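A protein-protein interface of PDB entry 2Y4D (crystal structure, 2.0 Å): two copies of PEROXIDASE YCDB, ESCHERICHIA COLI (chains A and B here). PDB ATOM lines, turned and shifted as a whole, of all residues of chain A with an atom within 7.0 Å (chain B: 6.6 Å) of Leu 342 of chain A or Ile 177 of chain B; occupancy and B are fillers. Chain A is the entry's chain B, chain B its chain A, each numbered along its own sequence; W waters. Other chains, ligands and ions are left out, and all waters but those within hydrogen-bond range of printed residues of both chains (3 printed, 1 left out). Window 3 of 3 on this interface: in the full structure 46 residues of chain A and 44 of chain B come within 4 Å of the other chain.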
ATOM      1  N   GLN A 256      14.557   8.064   3.187  1.00  0.00           N
ATOM      2  CA  GLN A 256      14.916   6.650   3.040  1.00  0.00           C
ATOM      3  C   GLN A 256      14.531   6.191   1.651  1.00  0.00           C
ATOM      4  O   GLN A 256      13.535   6.671   1.114  1.00  0.00           O
ATOM      5  CB  GLN A 256      14.174   5.744   4.054  1.00  0.00           C
ATOM      6  CG  GLN A 256      14.783   5.696   5.376  1.00  0.00           C
ATOM      7  CD  GLN A 256      14.051   4.766   6.351  1.00  0.00           C
ATOM      8  OE1 GLN A 256      13.083   4.088   6.004  1.00  0.00           O
ATOM      9  NE2 GLN A 256      14.536   4.731   7.565  1.00  0.00           N
ATOM     10  N   PHE A 257      15.296   5.256   1.102  1.00  0.00           N
ATOM     11  CA  PHE A 257      14.938   4.599  -0.162  1.00  0.00           C
ATOM     12  C   PHE A 257      14.633   3.141   0.083  1.00  0.00           C
ATOM     13  O   PHE A 257      15.360   2.449   0.825  1.00  0.00           O
ATOM     14  CB  PHE A 257      16.065   4.633  -1.206  1.00  0.00           C
ATOM     15  CG  PHE A 257      16.477   6.009  -1.647  1.00  0.00           C
ATOM     16  CD1 PHE A 257      15.662   7.110  -1.431  1.00  0.00           C
ATOM     17  CD2 PHE A 257      17.693   6.188  -2.323  1.00  0.00           C
ATOM     18  CE1 PHE A 257      16.044   8.364  -1.828  1.00  0.00           C
ATOM     19  CE2 PHE A 257      18.101   7.476  -2.740  1.00  0.00           C
ATOM     20  CZ  PHE A 257      17.259   8.565  -2.491  1.00  0.00           C
ATOM     21  N   ARG A 258      13.566   2.660  -0.541  1.00  0.00           N
ATOM     22  CA  ARG A 258      13.296   1.201  -0.567  1.00  0.00           C
ATOM     23  C   ARG A 258      14.171   0.578  -1.649  1.00  0.00           C
ATOM     24  O   ARG A 258      13.716   0.346  -2.789  1.00  0.00           O
ATOM     25  CB  ARG A 258      11.807   0.914  -0.809  1.00  0.00           C
ATOM     26  CG  ARG A 258      10.882   1.636   0.162  1.00  0.00           C
ATOM     27  CD  ARG A 258       9.404   1.328  -0.098  1.00  0.00           C
ATOM     28  NE  ARG A 258       8.658   1.790   1.070  1.00  0.00           N
ATOM     29  CZ  ARG A 258       8.088   2.988   1.201  1.00  0.00           C
ATOM     30  NH1 ARG A 258       8.088   3.872   0.201  1.00  0.00           N
ATOM     31  NH2 ARG A 258       7.474   3.285   2.340  1.00  0.00           N
ATOM     32  N   VAL A 259      15.426   0.296  -1.311  1.00  0.00           N
ATOM     33  CA  VAL A 259      16.386  -0.116  -2.350  1.00  0.00           C
ATOM     34  C   VAL A 259      16.211  -1.523  -2.891  1.00  0.00           C
ATOM     35  O   VAL A 259      16.401  -1.709  -4.082  1.00  0.00           O
ATOM     36  CB  VAL A 259      17.894   0.094  -1.986  1.00  0.00           C
ATOM     37  CG1 VAL A 259      18.241   1.615  -1.963  1.00  0.00           C
ATOM     38  CG2 VAL A 259      18.207  -0.566  -0.678  1.00  0.00           C
ATOM     39  N   GLU A 260      15.903  -2.496  -2.030  1.00  0.00           N
ATOM     40  CA  GLU A 260      15.736  -3.893  -2.502  1.00  0.00           C
ATOM     41  C   GLU A 260      14.603  -3.937  -3.542  1.00  0.00           C
ATOM     42  O   GLU A 260      14.771  -4.451  -4.651  1.00  0.00           O
ATOM     43  CB  GLU A 260      15.497  -4.867  -1.361  1.00  0.00           C
ATOM     44  CG  GLU A 260      16.614  -4.849  -0.339  1.00  0.00           C
ATOM     45  CD  GLU A 260      16.316  -3.959   0.861  1.00  0.00           C
ATOM     46  OE1 GLU A 260      15.593  -2.919   0.728  1.00  0.00           O
ATOM     47  OE2 GLU A 260      16.812  -4.289   1.957  1.00  0.00           O
ATOM     48  N   ASP A 263      15.550  -2.151  -6.789  1.00  0.00           N
ATOM     49  CA  ASP A 263      16.426  -3.015  -7.599  1.00  0.00           C
ATOM     50  C   ASP A 263      15.672  -4.177  -8.241  1.00  0.00           C
ATOM     51  O   ASP A 263      16.218  -4.836  -9.121  1.00  0.00           O
ATOM     52  CB  ASP A 263      17.618  -3.583  -6.796  1.00  0.00           C
ATOM     53  CG  ASP A 263      18.668  -2.495  -6.412  1.00  0.00           C
ATOM     54  OD1 ASP A 263      18.640  -1.377  -6.981  1.00  0.00           O
ATOM     55  OD2 ASP A 263      19.543  -2.787  -5.562  1.00  0.00           O
ATOM     56  N   SER A 333      24.112   5.720   4.138  1.00  0.00           N
ATOM     57  CA  SER A 333      23.917   4.300   4.253  1.00  0.00           C
ATOM     58  C   SER A 333      24.210   3.946   5.700  1.00  0.00           C
ATOM     59  O   SER A 333      25.310   4.193   6.185  1.00  0.00           O
ATOM     60  CB  SER A 333      24.813   3.541   3.254  1.00  0.00           C
ATOM     61  OG  SER A 333      24.701   2.112   3.337  1.00  0.00           O
ATOM     62  N   LEU A 334      23.222   3.384   6.402  1.00  0.00           N
ATOM     63  CA  LEU A 334      23.362   3.171   7.850  1.00  0.00           C
ATOM     64  C   LEU A 334      23.277   1.685   8.184  1.00  0.00           C
ATOM     65  O   LEU A 334      24.153   0.890   7.770  1.00  0.00           O
ATOM     66  CB  LEU A 334      22.301   4.017   8.597  1.00  0.00           C
ATOM     67  CG  LEU A 334      22.530   4.766   9.921  1.00  0.00           C
ATOM     68  CD1 LEU A 334      23.884   5.471  10.032  1.00  0.00           C
ATOM     69  CD2 LEU A 334      21.390   5.775  10.120  1.00  0.00           C
ATOM     70  N   GLY A 335      22.226   1.266   8.886  1.00  0.00           N
ATOM     71  CA  GLY A 335      22.084  -0.138   9.245  1.00  0.00           C
ATOM     72  C   GLY A 335      20.907  -0.747   8.477  1.00  0.00           C
ATOM     73  O   GLY A 335      20.886  -0.787   7.230  1.00  0.00           O
ATOM     74  N   VAL A 336      19.914  -1.174   9.244  1.00  0.00           N
ATOM     75  CA  VAL A 336      18.746  -1.838   8.741  1.00  0.00           C
ATOM     76  C   VAL A 336      17.549  -1.097   9.330  1.00  0.00           C
ATOM     77  O   VAL A 336      17.654  -0.536  10.413  1.00  0.00           O
ATOM     78  CB  VAL A 336      18.758  -3.293   9.227  1.00  0.00           C
ATOM     79  CG1 VAL A 336      17.628  -4.102   8.607  1.00  0.00           C
ATOM     80  CG2 VAL A 336      20.143  -3.983   8.931  1.00  0.00           C
ATOM     81  N   THR A 337      16.415  -1.076   8.624  1.00  0.00           N
ATOM     82  CA  THR A 337      15.191  -0.457   9.158  1.00  0.00           C
ATOM     83  C   THR A 337      14.481  -1.390  10.155  1.00  0.00           C
ATOM     84  O   THR A 337      14.803  -2.584  10.256  1.00  0.00           O
ATOM     85  CB  THR A 337      14.195  -0.137   8.017  1.00  0.00           C
ATOM     86  OG1 THR A 337      13.784  -1.373   7.408  1.00  0.00           O
ATOM     87  CG2 THR A 337      14.860   0.751   6.964  1.00  0.00           C
ATOM     88  N   GLY A 340      13.474  -4.491   8.779  1.00  0.00           N
ATOM     89  CA  GLY A 340      14.506  -5.444   8.356  1.00  0.00           C
ATOM     90  C   GLY A 340      15.072  -5.169   6.961  1.00  0.00           C
ATOM     91  O   GLY A 340      15.740  -6.005   6.389  1.00  0.00           O
ATOM     92  N   GLN A 341      14.811  -4.000   6.411  1.00  0.00           N
ATOM     93  CA  GLN A 341      15.325  -3.662   5.092  1.00  0.00           C
ATOM     94  C   GLN A 341      16.573  -2.784   5.212  1.00  0.00           C
ATOM     95  O   GLN A 341      16.819  -2.209   6.271  1.00  0.00           O
ATOM     96  CB  GLN A 341      14.255  -2.896   4.313  1.00  0.00           C
ATOM     97  CG  GLN A 341      12.959  -3.694   4.122  1.00  0.00           C
ATOM     98  CD  GLN A 341      13.165  -4.937   3.307  1.00  0.00           C
ATOM     99  OE1 GLN A 341      13.567  -5.976   3.823  1.00  0.00           O
ATOM    100  NE2 GLN A 341      12.872  -4.848   2.014  1.00  0.00           N
ATOM    101  N   LEU A 342      17.354  -2.676   4.137  1.00  0.00           N
ATOM    102  CA  LEU A 342      18.506  -1.755   4.169  1.00  0.00           C
ATOM    103  C   LEU A 342      18.072  -0.304   4.432  1.00  0.00           C
ATOM    104  O   LEU A 342      17.143   0.193   3.799  1.00  0.00           O
ATOM    105  CB  LEU A 342      19.302  -1.842   2.868  1.00  0.00           C
ATOM    106  CG  LEU A 342      19.899  -3.191   2.456  1.00  0.00           C
ATOM    107  CD1 LEU A 342      20.607  -3.006   1.110  1.00  0.00           C
ATOM    108  CD2 LEU A 342      20.839  -3.705   3.535  1.00  0.00           C
ATOM    109  N   ASP A 343      18.734   0.361   5.383  1.00  0.00           N
ATOM    110  CA  ASP A 343      18.513   1.772   5.653  1.00  0.00           C
ATOM    111  C   ASP A 343      19.541   2.573   4.824  1.00  0.00           C
ATOM    112  O   ASP A 343      20.729   2.643   5.186  1.00  0.00           O
ATOM    113  CB  ASP A 343      18.690   2.055   7.147  1.00  0.00           C
ATOM    114  CG  ASP A 343      18.252   3.471   7.533  1.00  0.00           C
ATOM    115  OD1 ASP A 343      17.905   4.285   6.651  1.00  0.00           O
ATOM    116  OD2 ASP A 343      18.247   3.764   8.738  1.00  0.00           O
ATOM    117  N   MET A 344      19.094   3.111   3.700  1.00  0.00           N
ATOM    118  CA  MET A 344      19.936   4.005   2.904  1.00  0.00           C
ATOM    119  C   MET A 344      19.077   4.954   2.119  1.00  0.00           C
ATOM    120  O   MET A 344      17.851   4.714   1.954  1.00  0.00           O
ATOM    121  CB  MET A 344      20.951   3.247   2.019  1.00  0.00           C
ATOM    122  CG  MET A 344      20.478   2.111   1.199  1.00  0.00           C
ATOM    123  SD  MET A 344      21.813   1.307   0.204  1.00  0.00           S
ATOM    124  CE  MET A 344      22.621   0.203   1.374  1.00  0.00           C
ATOM    125  N   GLY A 345      19.681   6.056   1.672  1.00  0.00           N
ATOM    126  CA  GLY A 345      18.896   7.101   1.088  1.00  0.00           C
ATOM    127  C   GLY A 345      19.637   8.362   0.752  1.00  0.00           C
ATOM    128  O   GLY A 345      20.790   8.336   0.358  1.00  0.00           O
ATOM    129  N   VAL B  55      28.125  -7.432   7.295  1.00  0.00           N
ATOM    130  CA  VAL B  55      26.682  -7.695   7.035  1.00  0.00           C
ATOM    131  C   VAL B  55      26.388  -9.142   7.359  1.00  0.00           C
ATOM    132  O   VAL B  55      26.922 -10.040   6.723  1.00  0.00           O
ATOM    133  CB  VAL B  55      26.271  -7.635   5.559  1.00  0.00           C
ATOM    134  CG1 VAL B  55      24.738  -7.459   5.424  1.00  0.00           C
ATOM    135  CG2 VAL B  55      27.068  -6.691   4.760  1.00  0.00           C
ATOM    136  N   PHE B  57      23.574 -12.280   7.685  1.00  0.00           N
ATOM    137  CA  PHE B  57      22.378 -12.721   6.982  1.00  0.00           C
ATOM    138  C   PHE B  57      21.773 -13.951   7.655  1.00  0.00           C
ATOM    139  O   PHE B  57      22.483 -14.774   8.209  1.00  0.00           O
ATOM    140  CB  PHE B  57      22.740 -13.167   5.570  1.00  0.00           C
ATOM    141  CG  PHE B  57      23.173 -12.058   4.645  1.00  0.00           C
ATOM    142  CD1 PHE B  57      22.234 -11.364   3.888  1.00  0.00           C
ATOM    143  CD2 PHE B  57      24.527 -11.704   4.538  1.00  0.00           C
ATOM    144  CE1 PHE B  57      22.628 -10.344   2.993  1.00  0.00           C
ATOM    145  CE2 PHE B  57      24.916 -10.661   3.660  1.00  0.00           C
ATOM    146  CZ  PHE B  57      23.973 -10.010   2.902  1.00  0.00           C
ATOM    147  N   ALA B 172      28.648  -3.710  -4.038  1.00  0.00           N
ATOM    148  CA  ALA B 172      28.807  -5.141  -3.861  1.00  0.00           C
ATOM    149  C   ALA B 172      27.643  -5.762  -3.083  1.00  0.00           C
ATOM    150  O   ALA B 172      27.105  -6.813  -3.485  1.00  0.00           O
ATOM    151  CB  ALA B 172      30.144  -5.484  -3.154  1.00  0.00           C
ATOM    152  N   LEU B 173      27.276  -5.127  -1.964  1.00  0.00           N
ATOM    153  CA  LEU B 173      26.201  -5.650  -1.133  1.00  0.00           C
ATOM    154  C   LEU B 173      24.916  -5.769  -1.984  1.00  0.00           C
ATOM    155  O   LEU B 173      24.215  -6.810  -1.993  1.00  0.00           O
ATOM    156  CB  LEU B 173      25.956  -4.744   0.094  1.00  0.00           C
ATOM    157  CG  LEU B 173      24.728  -5.172   0.939  1.00  0.00           C
ATOM    158  CD1 LEU B 173      24.899  -6.586   1.436  1.00  0.00           C
ATOM    159  CD2 LEU B 173      24.477  -4.220   2.097  1.00  0.00           C
ATOM    160  N   ARG B 174      24.628  -4.715  -2.711  1.00  0.00           N
ATOM    161  CA  ARG B 174      23.361  -4.679  -3.441  1.00  0.00           C
ATOM    162  C   ARG B 174      23.307  -5.673  -4.582  1.00  0.00           C
ATOM    163  O   ARG B 174      22.238  -6.276  -4.843  1.00  0.00           O
ATOM    164  CB  ARG B 174      23.055  -3.262  -3.876  1.00  0.00           C
ATOM    165  CG  ARG B 174      22.135  -2.662  -2.797  1.00  0.00           C
ATOM    166  CD  ARG B 174      21.871  -1.263  -2.978  1.00  0.00           C
ATOM    167  NE  ARG B 174      21.012  -0.949  -4.107  1.00  0.00           N
ATOM    168  CZ  ARG B 174      20.821   0.298  -4.482  1.00  0.00           C
ATOM    169  NH1 ARG B 174      21.455   1.268  -3.796  1.00  0.00           N
ATOM    170  NH2 ARG B 174      20.039   0.592  -5.511  1.00  0.00           N
ATOM    171  N   ASP B 175      24.467  -5.931  -5.191  1.00  0.00           N
ATOM    172  CA  ASP B 175      24.580  -6.979  -6.207  1.00  0.00           C
ATOM    173  C   ASP B 175      24.266  -8.347  -5.590  1.00  0.00           C
ATOM    174  O   ASP B 175      23.437  -9.138  -6.137  1.00  0.00           O
ATOM    175  CB  ASP B 175      25.966  -6.939  -6.884  1.00  0.00           C
ATOM    176  CG  ASP B 175      26.189  -8.119  -7.872  1.00  0.00           C
ATOM    177  OD1 ASP B 175      26.414  -9.261  -7.434  1.00  0.00           O
ATOM    178  OD2 ASP B 175      26.166  -7.864  -9.084  1.00  0.00           O
ATOM    179  N   ILE B 176      24.864  -8.600  -4.436  1.00  0.00           N
ATOM    180  CA  ILE B 176      24.667  -9.848  -3.706  1.00  0.00           C
ATOM    181  C   ILE B 176      23.191 -10.053  -3.283  1.00  0.00           C
ATOM    182  O   ILE B 176      22.596 -11.118  -3.554  1.00  0.00           O
ATOM    183  CB  ILE B 176      25.620  -9.939  -2.485  1.00  0.00           C
ATOM    184  CG1 ILE B 176      27.077  -9.978  -2.961  1.00  0.00           C
ATOM    185  CG2 ILE B 176      25.284 -11.144  -1.603  1.00  0.00           C
ATOM    186  CD1 ILE B 176      28.083  -9.403  -1.945  1.00  0.00           C
ATOM    187  N   ILE B 177      22.595  -9.032  -2.680  1.00  0.00           N
ATOM    188  CA  ILE B 177      21.157  -9.062  -2.328  1.00  0.00           C
ATOM    189  C   ILE B 177      20.214  -9.309  -3.555  1.00  0.00           C
ATOM    190  O   ILE B 177      19.326 -10.186  -3.501  1.00  0.00           O
ATOM    191  CB  ILE B 177      20.750  -7.789  -1.542  1.00  0.00           C
ATOM    192  CG1 ILE B 177      21.352  -7.862  -0.142  1.00  0.00           C
ATOM    193  CG2 ILE B 177      19.216  -7.692  -1.422  1.00  0.00           C
ATOM    194  CD1 ILE B 177      21.193  -6.557   0.669  1.00  0.00           C
ATOM    195  N   LYS B 178      20.438  -8.597  -4.658  1.00  0.00           N
ATOM    196  CA  LYS B 178      19.642  -8.772  -5.903  1.00  0.00           C
ATOM    197  C   LYS B 178      19.644 -10.212  -6.405  1.00  0.00           C
ATOM    198  O   LYS B 178      18.612 -10.737  -6.890  1.00  0.00           O
ATOM    199  CB  LYS B 178      20.150  -7.855  -7.017  1.00  0.00           C
ATOM    200  CG  LYS B 178      19.241  -7.778  -8.256  1.00  0.00           C
ATOM    201  CD  LYS B 178      20.012  -7.427  -9.518  1.00  0.00           C
ATOM    202  CE  LYS B 178      19.028  -7.248 -10.701  1.00  0.00           C
ATOM    203  NZ  LYS B 178      18.292  -8.502 -11.026  1.00  0.00           N
ATOM    204  N   HIS B 179      20.788 -10.869  -6.273  1.00  0.00           N
ATOM    205  CA  HIS B 179      20.936 -12.228  -6.753  1.00  0.00           C
ATOM    206  C   HIS B 179      20.443 -13.294  -5.775  1.00  0.00           C
ATOM    207  O   HIS B 179      20.438 -14.457  -6.138  1.00  0.00           O
ATOM    208  CB  HIS B 179      22.408 -12.510  -7.149  1.00  0.00           C
ATOM    209  CG  HIS B 179      22.806 -11.921  -8.471  1.00  0.00           C
ATOM    210  ND1 HIS B 179      23.267 -10.628  -8.602  1.00  0.00           N
ATOM    211  CD2 HIS B 179      22.811 -12.449  -9.723  1.00  0.00           C
ATOM    212  CE1 HIS B 179      23.520 -10.372  -9.877  1.00  0.00           C
ATOM    213  NE2 HIS B 179      23.265 -11.464 -10.578  1.00  0.00           N
ATOM    214  N   THR B 180      20.048 -12.928  -4.540  1.00  0.00           N
ATOM    215  CA  THR B 180      19.749 -13.923  -3.497  1.00  0.00           C
ATOM    216  C   THR B 180      18.416 -13.747  -2.735  1.00  0.00           C
ATOM    217  O   THR B 180      18.347 -14.125  -1.550  1.00  0.00           O
ATOM    218  CB  THR B 180      20.854 -13.960  -2.388  1.00  0.00           C
ATOM    219  OG1 THR B 180      21.035 -12.623  -1.903  1.00  0.00           O
ATOM    220  CG2 THR B 180      22.164 -14.529  -2.897  1.00  0.00           C
ATOM    221  N   PRO B 181      17.374 -13.189  -3.388  1.00  0.00           N
ATOM    222  CA  PRO B 181      16.153 -12.850  -2.656  1.00  0.00           C
ATOM    223  C   PRO B 181      15.476 -14.095  -2.054  1.00  0.00           C
ATOM    224  O   PRO B 181      14.723 -13.962  -1.106  1.00  0.00           O
ATOM    225  CB  PRO B 181      15.262 -12.172  -3.738  1.00  0.00           C
ATOM    226  CG  PRO B 181      15.688 -12.817  -5.005  1.00  0.00           C
ATOM    227  CD  PRO B 181      17.200 -12.964  -4.838  1.00  0.00           C
ATOM    228  N   ASP B 182      15.805 -15.288  -2.560  1.00  0.00           N
ATOM    229  CA  ASP B 182      15.202 -16.532  -2.096  1.00  0.00           C
ATOM    230  C   ASP B 182      16.144 -17.279  -1.164  1.00  0.00           C
ATOM    231  O   ASP B 182      15.826 -18.358  -0.673  1.00  0.00           O
ATOM    232  CB  ASP B 182      14.852 -17.438  -3.307  1.00  0.00           C
ATOM    233  CG  ASP B 182      16.093 -17.767  -4.170  1.00  0.00           C
ATOM    234  OD1 ASP B 182      16.989 -16.879  -4.329  1.00  0.00           O
ATOM    235  OD2 ASP B 182      16.184 -18.911  -4.681  1.00  0.00           O
ATOM    236  N   LEU B 184      18.952 -15.526   1.057  1.00  0.00           N
ATOM    237  CA  LEU B 184      19.538 -14.769   2.168  1.00  0.00           C
ATOM    238  C   LEU B 184      18.589 -13.653   2.551  1.00  0.00           C
ATOM    239  O   LEU B 184      17.947 -13.052   1.695  1.00  0.00           O
ATOM    240  CB  LEU B 184      20.848 -14.109   1.673  1.00  0.00           C
ATOM    241  CG  LEU B 184      22.046 -14.988   1.415  1.00  0.00           C
ATOM    242  CD1 LEU B 184      23.152 -14.053   0.876  1.00  0.00           C
ATOM    243  CD2 LEU B 184      22.488 -15.693   2.718  1.00  0.00           C
ATOM    244  N   VAL B 186      18.862 -10.096   5.031  1.00  0.00           N
ATOM    245  CA  VAL B 186      19.762  -9.242   5.855  1.00  0.00           C
ATOM    246  C   VAL B 186      19.321  -9.312   7.303  1.00  0.00           C
ATOM    247  O   VAL B 186      18.113  -9.111   7.612  1.00  0.00           O
ATOM    248  CB  VAL B 186      19.740  -7.756   5.420  1.00  0.00           C
ATOM    249  CG1 VAL B 186      20.708  -6.922   6.293  1.00  0.00           C
ATOM    250  CG2 VAL B 186      20.228  -7.644   4.020  1.00  0.00           C
ATOM    251  N   LYS B 189      23.647  -5.054   9.988  1.00  0.00           N
ATOM    252  CA  LYS B 189      24.709  -4.499   9.140  1.00  0.00           C
ATOM    253  C   LYS B 189      25.283  -3.250   9.769  1.00  0.00           C
ATOM    254  O   LYS B 189      24.531  -2.430  10.325  1.00  0.00           O
ATOM    255  CB  LYS B 189      24.116  -4.124   7.776  1.00  0.00           C
ATOM    256  CG  LYS B 189      24.977  -3.251   6.814  1.00  0.00           C
ATOM    257  CD  LYS B 189      24.054  -2.704   5.734  1.00  0.00           C
ATOM    258  CE  LYS B 189      24.686  -1.634   4.792  1.00  0.00           C
ATOM    259  NZ  LYS B 189      24.819  -0.271   5.405  1.00  0.00           N
HETATM  260  O   HOH W   1      15.707  -8.628   6.436  1.00  0.00           O
HETATM  261  O   HOH W   2      22.010   0.160   4.768  1.00  0.00           O
HETATM  262  O   HOH W   3      19.673  -5.094  -4.170  1.00  0.00           O
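The guanidinium group (NE) of Arg 174 of chain B lies within salt-bridge range of the side-chain carboxylate (OD2) of Asp 263 of chain A (2.8 Å). The side-chain hydroxyl (OG) of Ser 333 of chain A is in hydrogen-bond range of the side-chain amino group (NZ) of Lys 189 of chain B (3.2 Å). The side-chain amino group of Lys 189 of chain B lies within hydrogen-bond range of the backbone carbonyl oxygen of Leu 334 of chain A, 2.7 Å away.
The backbone carbonyl oxygen (O) of Ile 177 of chain B is in hydrogen-bond range of the side-chain hydroxyl (OG1) of Thr 180 of chain B (3.4 Å). The backbone NH of Leu 342 of chain A lies within hydrogen-bond range of the side-chain carboxylate of Glu 260 of chain A, at 2.8 Å. N of Leu 334 of chain A lies within hydrogen-bond range of O of Asp 343 of chain A (2.9 Å). The backbone carbonyl oxygen (O) of Gly 335 of chain A sits at hydrogen-bond distance from the backbone NH (N) of Asp 343 of chain A, 3.1 Å away.
Val 259 of chain A touches Arg 174 of chain B (CG1 to NH1, 3.7 Å). Lys 189 of chain B touches Gly 335 of chain A. Val 336 of chain A touches Val 186 of chain B (CG2 to CG1, 3.99 Å). CG2 of Val 336 of chain A touches N of Lys 189 of chain B, 3.8 Å away. CD2 of Leu 342 of chain A touches CD2 of Leu 173 of chain B (3.9 Å). CD1 of Ile 177 of chain B touches CD1 of Leu 342 of chain A, at 3.6 Å.
Of the printed residues of chain B, Leu 342 of chain A touches Leu 173 and Ile 177. Printed residues of chain A within 4 Å of Ile 177 of chain B: Leu 342. Of the printed residues of chain A, Lys 189 of chain B touches Ser 333, Leu 334, Gly 335 and Val 336. Of the printed residues of chain B, Asp 263 of chain A touches Arg 174. Of the printed residues of chain B, Gly 335 of chain A touches Lys 189. Printed residues of chain A within 4 Å of Val 186 of chain B: Val 336. Of the printed residues of chain A, Arg 174 of chain B touches Val 259 (3.7 Å) and Asp 263 (2.8 Å). The nearest printed residue of chain A that does not touch Ile 177 of chain B is Glu 260 of chain A (4.003 Å).
Hydrophobic or aromatic side chains of chain A that line the printed part of chain B: Val 259, Val 336 and Leu 342. Among the printed residues, 9 pairs touch across the chains. Among the printed residues, Asp or Glu carboxylates within 4 Å of a Lys or Arg side-chain nitrogen of the other chain: Asp 263 of chain A with Arg 174 of chain B.
No position is printed for both chains. Of the 9 pairs that touch across the chains among the printed residues, none has its exchanged pair printed and touching as well.
Water W1 lies within hydrogen-bond range of O of Gly 340 of chain A (2.6 Å) and O of Val 186 of chain B (2.7 Å). Water W3 bridges OD2 of Asp 263 of chain A (2.7 Å) and O of Arg 174 of chain B (2.9 Å). Water W2 lies within hydrogen-bond range of O of Asp 343 of chain A (2.8 Å), O of Gly 335 of chain A (2.9 Å) and NZ of Lys 189 of chain B (2.9 Å).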
